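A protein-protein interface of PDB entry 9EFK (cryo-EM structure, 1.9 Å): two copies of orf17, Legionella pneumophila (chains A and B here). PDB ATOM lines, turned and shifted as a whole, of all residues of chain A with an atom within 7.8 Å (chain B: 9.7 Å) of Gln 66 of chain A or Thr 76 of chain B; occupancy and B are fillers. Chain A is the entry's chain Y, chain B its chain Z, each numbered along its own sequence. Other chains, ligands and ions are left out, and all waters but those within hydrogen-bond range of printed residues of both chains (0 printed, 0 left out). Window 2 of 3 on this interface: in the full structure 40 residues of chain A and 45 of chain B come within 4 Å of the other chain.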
ATOM      1  N   PHE A  64      11.217  13.685 -15.226  1.00  0.00           N
ATOM      2  CA  PHE A  64       9.986  13.758 -14.457  1.00  0.00           C
ATOM      3  C   PHE A  64       9.342  12.382 -14.393  1.00  0.00           C
ATOM      4  O   PHE A  64       9.552  11.533 -15.259  1.00  0.00           O
ATOM      5  CB  PHE A  64       9.003  14.775 -15.049  1.00  0.00           C
ATOM      6  CG  PHE A  64       8.353  14.322 -16.318  1.00  0.00           C
ATOM      7  CD1 PHE A  64       8.956  14.550 -17.538  1.00  0.00           C
ATOM      8  CD2 PHE A  64       7.130  13.679 -16.292  1.00  0.00           C
ATOM      9  CE1 PHE A  64       8.358  14.135 -18.703  1.00  0.00           C
ATOM     10  CE2 PHE A  64       6.535  13.257 -17.452  1.00  0.00           C
ATOM     11  CZ  PHE A  64       7.144  13.490 -18.659  1.00  0.00           C
ATOM     12  N   GLN A  65       8.542  12.180 -13.351  1.00  0.00           N
ATOM     13  CA  GLN A  65       7.888  10.901 -13.123  1.00  0.00           C
ATOM     14  C   GLN A  65       6.711  11.114 -12.187  1.00  0.00           C
ATOM     15  O   GLN A  65       6.833  11.824 -11.189  1.00  0.00           O
ATOM     16  CB  GLN A  65       8.866   9.889 -12.523  1.00  0.00           C
ATOM     17  CG  GLN A  65       8.299   8.505 -12.353  1.00  0.00           C
ATOM     18  CD  GLN A  65       9.260   7.573 -11.658  1.00  0.00           C
ATOM     19  OE1 GLN A  65      10.469   7.795 -11.659  1.00  0.00           O
ATOM     20  NE2 GLN A  65       8.727   6.524 -11.051  1.00  0.00           N
ATOM     21  N   GLN A  66       5.580  10.497 -12.509  1.00  0.00           N
ATOM     22  CA  GLN A  66       4.413  10.569 -11.642  1.00  0.00           C
ATOM     23  C   GLN A  66       4.532   9.582 -10.491  1.00  0.00           C
ATOM     24  O   GLN A  66       4.927   8.430 -10.678  1.00  0.00           O
ATOM     25  CB  GLN A  66       3.133  10.292 -12.427  1.00  0.00           C
ATOM     26  CG  GLN A  66       2.619  11.484 -13.199  1.00  0.00           C
ATOM     27  CD  GLN A  66       1.127  11.420 -13.440  1.00  0.00           C
ATOM     28  OE1 GLN A  66       0.515  10.360 -13.338  1.00  0.00           O
ATOM     29  NE2 GLN A  66       0.530  12.561 -13.751  1.00  0.00           N
ATOM     30  N   ILE A  67       4.187  10.047  -9.295  1.00  0.00           N
ATOM     31  CA  ILE A  67       4.175   9.230  -8.089  1.00  0.00           C
ATOM     32  C   ILE A  67       2.722   9.007  -7.700  1.00  0.00           C
ATOM     33  O   ILE A  67       1.974   9.967  -7.492  1.00  0.00           O
ATOM     34  CB  ILE A  67       4.951   9.894  -6.942  1.00  0.00           C
ATOM     35  CG1 ILE A  67       6.367  10.266  -7.387  1.00  0.00           C
ATOM     36  CG2 ILE A  67       4.991   8.983  -5.728  1.00  0.00           C
ATOM     37  CD1 ILE A  67       7.179   9.107  -7.882  1.00  0.00           C
ATOM     38  N   SER A  68       2.319   7.743  -7.607  1.00  0.00           N
ATOM     39  CA  SER A  68       0.952   7.400  -7.254  1.00  0.00           C
ATOM     40  C   SER A  68       0.831   6.506  -6.032  1.00  0.00           C
ATOM     41  O   SER A  68      -0.216   6.530  -5.380  1.00  0.00           O
ATOM     42  CB  SER A  68       0.248   6.718  -8.437  1.00  0.00           C
ATOM     43  OG  SER A  68       0.921   5.532  -8.806  1.00  0.00           O
ATOM     44  N   ILE A  69       1.858   5.730  -5.700  1.00  0.00           N
ATOM     45  CA  ILE A  69       1.815   4.863  -4.530  1.00  0.00           C
ATOM     46  C   ILE A  69       2.128   5.693  -3.295  1.00  0.00           C
ATOM     47  O   ILE A  69       3.293   5.874  -2.930  1.00  0.00           O
ATOM     48  CB  ILE A  69       2.796   3.686  -4.666  1.00  0.00           C
ATOM     49  CG1 ILE A  69       2.561   2.949  -5.982  1.00  0.00           C
ATOM     50  CG2 ILE A  69       2.640   2.735  -3.497  1.00  0.00           C
ATOM     51  CD1 ILE A  69       1.201   2.325  -6.086  1.00  0.00           C
ATOM     52  N   PRO A  87      11.801   7.341  -6.139  1.00  0.00           N
ATOM     53  CA  PRO A  87      12.121   6.322  -7.145  1.00  0.00           C
ATOM     54  C   PRO A  87      13.614   6.046  -7.224  1.00  0.00           C
ATOM     55  O   PRO A  87      14.446   6.920  -6.980  1.00  0.00           O
ATOM     56  CB  PRO A  87      11.590   6.928  -8.449  1.00  0.00           C
ATOM     57  CG  PRO A  87      11.330   8.363  -8.148  1.00  0.00           C
ATOM     58  CD  PRO A  87      11.004   8.438  -6.702  1.00  0.00           C
ATOM     59  N   TYR A  97       5.284  18.884  -8.572  1.00  0.00           N
ATOM     60  CA  TYR A  97       4.141  19.547  -9.173  1.00  0.00           C
ATOM     61  C   TYR A  97       2.902  18.699  -8.918  1.00  0.00           C
ATOM     62  O   TYR A  97       2.942  17.478  -9.117  1.00  0.00           O
ATOM     63  CB  TYR A  97       4.325  19.768 -10.677  1.00  0.00           C
ATOM     64  CG  TYR A  97       3.119  20.405 -11.323  1.00  0.00           C
ATOM     65  CD1 TYR A  97       2.974  21.781 -11.349  1.00  0.00           C
ATOM     66  CD2 TYR A  97       2.120  19.632 -11.892  1.00  0.00           C
ATOM     67  CE1 TYR A  97       1.876  22.367 -11.927  1.00  0.00           C
ATOM     68  CE2 TYR A  97       1.017  20.211 -12.471  1.00  0.00           C
ATOM     69  CZ  TYR A  97       0.902  21.578 -12.487  1.00  0.00           C
ATOM     70  OH  TYR A  97      -0.196  22.161 -13.067  1.00  0.00           O
ATOM     71  N   PRO A  98       1.787  19.295  -8.489  1.00  0.00           N
ATOM     72  CA  PRO A  98       1.579  20.716  -8.185  1.00  0.00           C
ATOM     73  C   PRO A  98       2.254  21.132  -6.886  1.00  0.00           C
ATOM     74  O   PRO A  98       2.949  20.342  -6.262  1.00  0.00           O
ATOM     75  CB  PRO A  98       0.053  20.825  -8.109  1.00  0.00           C
ATOM     76  CG  PRO A  98      -0.384  19.483  -7.642  1.00  0.00           C
ATOM     77  CD  PRO A  98       0.545  18.521  -8.323  1.00  0.00           C
ATOM     78  N   THR A 116      -2.088  12.017  -6.665  1.00  0.00           N
ATOM     79  CA  THR A 116      -0.918  11.815  -7.505  1.00  0.00           C
ATOM     80  C   THR A 116      -0.247  13.148  -7.810  1.00  0.00           C
ATOM     81  O   THR A 116      -0.912  14.146  -8.093  1.00  0.00           O
ATOM     82  CB  THR A 116      -1.326  11.116  -8.804  1.00  0.00           C
ATOM     83  OG1 THR A 116      -1.811   9.803  -8.508  1.00  0.00           O
ATOM     84  CG2 THR A 116      -0.156  11.003  -9.761  1.00  0.00           C
ATOM     85  N   PHE A 117       1.080  13.162  -7.737  1.00  0.00           N
ATOM     86  CA  PHE A 117       1.873  14.328  -8.085  1.00  0.00           C
ATOM     87  C   PHE A 117       3.029  13.895  -8.975  1.00  0.00           C
ATOM     88  O   PHE A 117       3.269  12.707  -9.182  1.00  0.00           O
ATOM     89  CB  PHE A 117       2.393  15.051  -6.837  1.00  0.00           C
ATOM     90  CG  PHE A 117       3.238  14.193  -5.946  1.00  0.00           C
ATOM     91  CD1 PHE A 117       4.603  14.112  -6.133  1.00  0.00           C
ATOM     92  CD2 PHE A 117       2.667  13.467  -4.921  1.00  0.00           C
ATOM     93  CE1 PHE A 117       5.381  13.324  -5.320  1.00  0.00           C
ATOM     94  CE2 PHE A 117       3.444  12.678  -4.102  1.00  0.00           C
ATOM     95  CZ  PHE A 117       4.800  12.609  -4.302  1.00  0.00           C
ATOM     96  N   THR A 118       3.749  14.878  -9.495  1.00  0.00           N
ATOM     97  CA  THR A 118       4.893  14.652 -10.361  1.00  0.00           C
ATOM     98  C   THR A 118       6.165  15.093  -9.654  1.00  0.00           C
ATOM     99  O   THR A 118       6.204  16.156  -9.030  1.00  0.00           O
ATOM    100  CB  THR A 118       4.746  15.410 -11.682  1.00  0.00           C
ATOM    101  OG1 THR A 118       3.572  14.960 -12.360  1.00  0.00           O
ATOM    102  CG2 THR A 118       5.947  15.171 -12.570  1.00  0.00           C
ATOM    103  N   LEU A 119       7.195  14.266  -9.743  1.00  0.00           N
ATOM    104  CA  LEU A 119       8.502  14.575  -9.191  1.00  0.00           C
ATOM    105  C   LEU A 119       9.431  15.020 -10.310  1.00  0.00           C
ATOM    106  O   LEU A 119       9.568  14.326 -11.318  1.00  0.00           O
ATOM    107  CB  LEU A 119       9.079  13.358  -8.472  1.00  0.00           C
ATOM    108  CG  LEU A 119      10.534  13.439  -8.026  1.00  0.00           C
ATOM    109  CD1 LEU A 119      10.700  14.464  -6.927  1.00  0.00           C
ATOM    110  CD2 LEU A 119      11.016  12.082  -7.576  1.00  0.00           C
ATOM    111  N   ILE A 120      10.056  16.180 -10.135  1.00  0.00           N
ATOM    112  CA  ILE A 120      11.097  16.665 -11.032  1.00  0.00           C
ATOM    113  C   ILE A 120      12.437  16.399 -10.367  1.00  0.00           C
ATOM    114  O   ILE A 120      12.659  16.818  -9.227  1.00  0.00           O
ATOM    115  CB  ILE A 120      10.928  18.162 -11.336  1.00  0.00           C
ATOM    116  CG1 ILE A 120       9.508  18.463 -11.806  1.00  0.00           C
ATOM    117  CG2 ILE A 120      11.947  18.609 -12.365  1.00  0.00           C
ATOM    118  CD1 ILE A 120       9.170  17.843 -13.107  1.00  0.00           C
ATOM    119  N   TYR A 121      13.336  15.722 -11.072  1.00  0.00           N
ATOM    120  CA  TYR A 121      14.546  15.232 -10.434  1.00  0.00           C
ATOM    121  C   TYR A 121      15.673  15.123 -11.450  1.00  0.00           C
ATOM    122  O   TYR A 121      15.461  15.194 -12.659  1.00  0.00           O
ATOM    123  CB  TYR A 121      14.297  13.883  -9.761  1.00  0.00           C
ATOM    124  CG  TYR A 121      13.933  12.766 -10.710  1.00  0.00           C
ATOM    125  CD1 TYR A 121      12.639  12.622 -11.181  1.00  0.00           C
ATOM    126  CD2 TYR A 121      14.879  11.848 -11.124  1.00  0.00           C
ATOM    127  CE1 TYR A 121      12.303  11.604 -12.037  1.00  0.00           C
ATOM    128  CE2 TYR A 121      14.552  10.823 -11.976  1.00  0.00           C
ATOM    129  CZ  TYR A 121      13.263  10.707 -12.433  1.00  0.00           C
ATOM    130  OH  TYR A 121      12.935   9.686 -13.287  1.00  0.00           O
ATOM    131  N   THR B  72       3.128  10.604 -28.569  1.00  0.00           N
ATOM    132  CA  THR B  72       2.928   9.753 -27.396  1.00  0.00           C
ATOM    133  C   THR B  72       3.706  10.197 -26.162  1.00  0.00           C
ATOM    134  O   THR B  72       3.684   9.482 -25.157  1.00  0.00           O
ATOM    135  CB  THR B  72       3.258   8.273 -27.662  1.00  0.00           C
ATOM    136  OG1 THR B  72       4.672   8.061 -27.585  1.00  0.00           O
ATOM    137  CG2 THR B  72       2.750   7.832 -29.030  1.00  0.00           C
ATOM    138  N   LEU B  73       4.376  11.344 -26.184  1.00  0.00           N
ATOM    139  CA  LEU B  73       5.102  11.845 -25.024  1.00  0.00           C
ATOM    140  C   LEU B  73       4.369  13.057 -24.466  1.00  0.00           C
ATOM    141  O   LEU B  73       4.113  14.019 -25.197  1.00  0.00           O
ATOM    142  CB  LEU B  73       6.542  12.204 -25.383  1.00  0.00           C
ATOM    143  CG  LEU B  73       7.411  11.075 -25.934  1.00  0.00           C
ATOM    144  CD1 LEU B  73       8.827  11.562 -26.151  1.00  0.00           C
ATOM    145  CD2 LEU B  73       7.394   9.874 -25.011  1.00  0.00           C
ATOM    146  N   ASN B  74       4.039  13.011 -23.181  1.00  0.00           N
ATOM    147  CA  ASN B  74       3.257  14.061 -22.529  1.00  0.00           C
ATOM    148  C   ASN B  74       3.964  14.522 -21.262  1.00  0.00           C
ATOM    149  O   ASN B  74       4.087  13.731 -20.304  1.00  0.00           O
ATOM    150  CB  ASN B  74       1.853  13.557 -22.219  1.00  0.00           C
ATOM    151  CG  ASN B  74       1.221  12.848 -23.397  1.00  0.00           C
ATOM    152  OD1 ASN B  74       0.965  11.646 -23.348  1.00  0.00           O
ATOM    153  ND2 ASN B  74       0.973  13.588 -24.469  1.00  0.00           N
ATOM    154  N   PRO B  75       4.437  15.770 -21.210  1.00  0.00           N
ATOM    155  CA  PRO B  75       5.250  16.209 -20.061  1.00  0.00           C
ATOM    156  C   PRO B  75       4.558  16.145 -18.707  1.00  0.00           C
ATOM    157  O   PRO B  75       5.238  15.905 -17.704  1.00  0.00           O
ATOM    158  CB  PRO B  75       5.614  17.648 -20.440  1.00  0.00           C
ATOM    159  CG  PRO B  75       5.582  17.656 -21.915  1.00  0.00           C
ATOM    160  CD  PRO B  75       4.483  16.732 -22.318  1.00  0.00           C
ATOM    161  N   THR B  76       3.258  16.417 -18.627  1.00  0.00           N
ATOM    162  CA  THR B  76       2.411  16.223 -17.445  1.00  0.00           C
ATOM    163  C   THR B  76       2.698  17.174 -16.272  1.00  0.00           C
ATOM    164  O   THR B  76       1.941  17.157 -15.295  1.00  0.00           O
ATOM    165  CB  THR B  76       2.460  14.763 -16.945  1.00  0.00           C
ATOM    166  OG1 THR B  76       1.139  14.322 -16.612  1.00  0.00           O
ATOM    167  CG2 THR B  76       3.361  14.593 -15.723  1.00  0.00           C
ATOM    168  N   PHE B  77       3.711  18.038 -16.345  1.00  0.00           N
ATOM    169  CA  PHE B  77       4.007  18.949 -15.245  1.00  0.00           C
ATOM    170  C   PHE B  77       4.124  20.381 -15.746  1.00  0.00           C
ATOM    171  O   PHE B  77       4.500  20.625 -16.894  1.00  0.00           O
ATOM    172  CB  PHE B  77       5.299  18.562 -14.507  1.00  0.00           C
ATOM    173  CG  PHE B  77       6.553  18.890 -15.260  1.00  0.00           C
ATOM    174  CD1 PHE B  77       7.057  18.017 -16.204  1.00  0.00           C
ATOM    175  CD2 PHE B  77       7.235  20.069 -15.018  1.00  0.00           C
ATOM    176  CE1 PHE B  77       8.206  18.317 -16.894  1.00  0.00           C
ATOM    177  CE2 PHE B  77       8.381  20.371 -15.706  1.00  0.00           C
ATOM    178  CZ  PHE B  77       8.867  19.496 -16.644  1.00  0.00           C
ATOM    179  N   ASP B  78       3.797  21.324 -14.862  1.00  0.00           N
ATOM    180  CA  ASP B  78       3.935  22.764 -15.088  1.00  0.00           C
ATOM    181  C   ASP B  78       3.164  23.255 -16.306  1.00  0.00           C
ATOM    182  O   ASP B  78       3.465  24.324 -16.839  1.00  0.00           O
ATOM    183  CB  ASP B  78       5.405  23.176 -15.215  1.00  0.00           C
ATOM    184  CG  ASP B  78       6.094  23.309 -13.875  1.00  0.00           C
ATOM    185  OD1 ASP B  78       5.405  23.581 -12.875  1.00  0.00           O
ATOM    186  OD2 ASP B  78       7.327  23.147 -13.822  1.00  0.00           O
ATOM    187  N   GLY B  79       2.167  22.508 -16.765  1.00  0.00           N
ATOM    188  CA  GLY B  79       1.389  22.926 -17.907  1.00  0.00           C
ATOM    189  C   GLY B  79       2.016  22.670 -19.258  1.00  0.00           C
ATOM    190  O   GLY B  79       1.434  23.070 -20.272  1.00  0.00           O
ATOM    191  N   TRP B  80       3.177  22.027 -19.314  1.00  0.00           N
ATOM    192  CA  TRP B  80       3.785  21.696 -20.595  1.00  0.00           C
ATOM    193  C   TRP B  80       2.991  20.598 -21.286  1.00  0.00           C
ATOM    194  O   TRP B  80       2.522  19.654 -20.647  1.00  0.00           O
ATOM    195  CB  TRP B  80       5.234  21.261 -20.400  1.00  0.00           C
ATOM    196  CG  TRP B  80       6.075  22.307 -19.762  1.00  0.00           C
ATOM    197  CD1 TRP B  80       6.602  22.281 -18.511  1.00  0.00           C
ATOM    198  CD2 TRP B  80       6.475  23.551 -20.340  1.00  0.00           C
ATOM    199  NE1 TRP B  80       7.310  23.428 -18.271  1.00  0.00           N
ATOM    200  CE2 TRP B  80       7.249  24.226 -19.380  1.00  0.00           C
ATOM    201  CE3 TRP B  80       6.254  24.161 -21.575  1.00  0.00           C
ATOM    202  CZ2 TRP B  80       7.801  25.477 -19.617  1.00  0.00           C
ATOM    203  CZ3 TRP B  80       6.807  25.397 -21.808  1.00  0.00           C
ATOM    204  CH2 TRP B  80       7.571  26.043 -20.837  1.00  0.00           C
ATOM    205  N   LEU B  81       2.839  20.722 -22.603  1.00  0.00           N
ATOM    206  CA  LEU B  81       1.999  19.816 -23.372  1.00  0.00           C
ATOM    207  C   LEU B  81       2.755  18.931 -24.348  1.00  0.00           C
ATOM    208  O   LEU B  81       2.334  17.797 -24.572  1.00  0.00           O
ATOM    209  CB  LEU B  81       0.941  20.604 -24.152  1.00  0.00           C
ATOM    210  CG  LEU B  81      -0.051  21.402 -23.309  1.00  0.00           C
ATOM    211  CD1 LEU B  81      -1.056  22.103 -24.196  1.00  0.00           C
ATOM    212  CD2 LEU B  81      -0.754  20.495 -22.322  1.00  0.00           C
ATOM    213  N   TYR B  82       3.856  19.402 -24.928  1.00  0.00           N
ATOM    214  CA  TYR B  82       4.544  18.668 -25.978  1.00  0.00           C
ATOM    215  C   TYR B  82       6.038  18.605 -25.706  1.00  0.00           C
ATOM    216  O   TYR B  82       6.613  19.497 -25.081  1.00  0.00           O
ATOM    217  CB  TYR B  82       4.314  19.306 -27.348  1.00  0.00           C
ATOM    218  CG  TYR B  82       2.863  19.552 -27.665  1.00  0.00           C
ATOM    219  CD1 TYR B  82       2.044  18.520 -28.088  1.00  0.00           C
ATOM    220  CD2 TYR B  82       2.313  20.814 -27.538  1.00  0.00           C
ATOM    221  CE1 TYR B  82       0.719  18.739 -28.373  1.00  0.00           C
ATOM    222  CE2 TYR B  82       0.992  21.043 -27.823  1.00  0.00           C
ATOM    223  CZ  TYR B  82       0.199  20.001 -28.240  1.00  0.00           C
ATOM    224  OH  TYR B  82      -1.124  20.225 -28.526  1.00  0.00           O
ATOM    225  N   GLU B  83       6.661  17.536 -26.192  1.00  0.00           N
ATOM    226  CA  GLU B  83       8.106  17.378 -26.185  1.00  0.00           C
ATOM    227  C   GLU B  83       8.593  17.354 -27.623  1.00  0.00           C
ATOM    228  O   GLU B  83       8.078  16.595 -28.446  1.00  0.00           O
ATOM    229  CB  GLU B  83       8.529  16.095 -25.469  1.00  0.00           C
ATOM    230  CG  GLU B  83       7.777  15.833 -24.184  1.00  0.00           C
ATOM    231  CD  GLU B  83       8.446  14.797 -23.306  1.00  0.00           C
ATOM    232  OE1 GLU B  83       8.312  14.890 -22.070  1.00  0.00           O
ATOM    233  OE2 GLU B  83       9.109  13.892 -23.847  1.00  0.00           O
ATOM    234  N   PHE B 105      14.453  20.692 -21.355  1.00  0.00           N
ATOM    235  CA  PHE B 105      14.246  19.744 -20.267  1.00  0.00           C
ATOM    236  C   PHE B 105      14.710  18.378 -20.740  1.00  0.00           C
ATOM    237  O   PHE B 105      14.151  17.830 -21.692  1.00  0.00           O
ATOM    238  CB  PHE B 105      12.774  19.713 -19.853  1.00  0.00           C
ATOM    239  CG  PHE B 105      12.520  19.031 -18.546  1.00  0.00           C
ATOM    240  CD1 PHE B 105      12.306  17.666 -18.493  1.00  0.00           C
ATOM    241  CD2 PHE B 105      12.478  19.756 -17.373  1.00  0.00           C
ATOM    242  CE1 PHE B 105      12.065  17.040 -17.295  1.00  0.00           C
ATOM    243  CE2 PHE B 105      12.239  19.134 -16.173  1.00  0.00           C
ATOM    244  CZ  PHE B 105      12.031  17.774 -16.135  1.00  0.00           C
ATOM    245  N   LEU B 110      10.329  21.553 -24.322  1.00  0.00           N
ATOM    246  CA  LEU B 110       8.925  21.488 -23.953  1.00  0.00           C
ATOM    247  C   LEU B 110       8.211  22.757 -24.393  1.00  0.00           C
ATOM    248  O   LEU B 110       8.732  23.861 -24.235  1.00  0.00           O
ATOM    249  CB  LEU B 110       8.776  21.291 -22.446  1.00  0.00           C
ATOM    250  CG  LEU B 110       9.533  20.106 -21.845  1.00  0.00           C
ATOM    251  CD1 LEU B 110       9.178  19.931 -20.386  1.00  0.00           C
ATOM    252  CD2 LEU B 110       9.252  18.836 -22.612  1.00  0.00           C
ATOM    253  N   THR B 111       7.021  22.592 -24.963  1.00  0.00           N
ATOM    254  CA  THR B 111       6.222  23.719 -25.421  1.00  0.00           C
ATOM    255  C   THR B 111       4.780  23.522 -24.980  1.00  0.00           C
ATOM    256  O   THR B 111       4.381  22.438 -24.550  1.00  0.00           O
ATOM    257  CB  THR B 111       6.282  23.892 -26.944  1.00  0.00           C
ATOM    258  OG1 THR B 111       5.740  22.729 -27.577  1.00  0.00           O
ATOM    259  CG2 THR B 111       7.710  24.095 -27.413  1.00  0.00           C
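NE2 of Gln 66 of chain A sits at hydrogen-bond distance from OG1 of Thr 76 of chain B (3.4 Å).
Printed residues of chain A that touch a printed residue of chain B: Phe 64, Gln 66, Tyr 97, Thr 118 and Ile 120. Hydrophobic or aromatic side chains of chain B that line the printed part of chain A: Phe 77 and Phe 105. Along chain B the printed residues that touch a printed residue of chain A span positions 74 to 105. Among the printed residues, no Asp or Glu carboxylate lies within 4 Å of a Lys or Arg side-chain nitrogen of the other chain.
No position is printed for both chains.
The backbone NH of Thr 118 of chain A sits at hydrogen-bond distance from the backbone carbonyl oxygen of Tyr 97 of chain A (2.7 Å).
O of Asn 74 of chain B touches CZ of Phe 64 of chain A (3.5 Å). CE2 of Phe 64 of chain A touches O of Pro 75 of chain B, at 3.0 Å. Phe 77 of chain B touches Phe 64 of chain A (CE1 to CD1, 3.9 Å). OE1 of Glu 83 of chain B touches CE1 of Phe 64 of chain A (3.5 Å). CE1 of Phe 105 of chain B touches CD1 of Phe 64 of chain A, 3.99 Å away. Tyr 97 of chain A touches Phe 77 of chain B. OD1 of Asp 78 of chain B touches CD1 of Tyr 97 of chain A, at 3.4 Å. CG2 of Thr 118 of chain A touches CB of Phe 77 of chain B, at 3.96 Å. CD1 of Ile 120 of chain A touches CD2 of Phe 77 of chain B (3.5 Å). Phe 105 of chain B touches Ile 120 of chain A.
Gln 66 of chain A touches just one residue of chain B: Thr 76. No residue of chain B comes within 4 Å of Ile 67 of chain A. Printed residues of chain B within 4 Å of Tyr 97 of chain A: Phe 77 (3.9 Å) and Asp 78 (3.4 Å). Pro 98 of chain A touches none of the printed residues of chain B. Of chain A, only Phe 64 (3.9 Å), Gln 66 (3.4 Å) and Thr 118 (3.4 Å) come within 4 Å of Thr 76 of chain B. Of the printed residues of chain A, Glu 83 of chain B touches Phe 64 (3.5 Å). Leu 110 of chain B touches none of the printed residues of chain A. The nearest printed residue of chain B that does not touch Gln 66 of chain A is Pro 75 of chain B (6.8 Å). The nearest residue of chain A that does not touch Thr 76 of chain B is Tyr 97 of chain A (4.2 Å).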
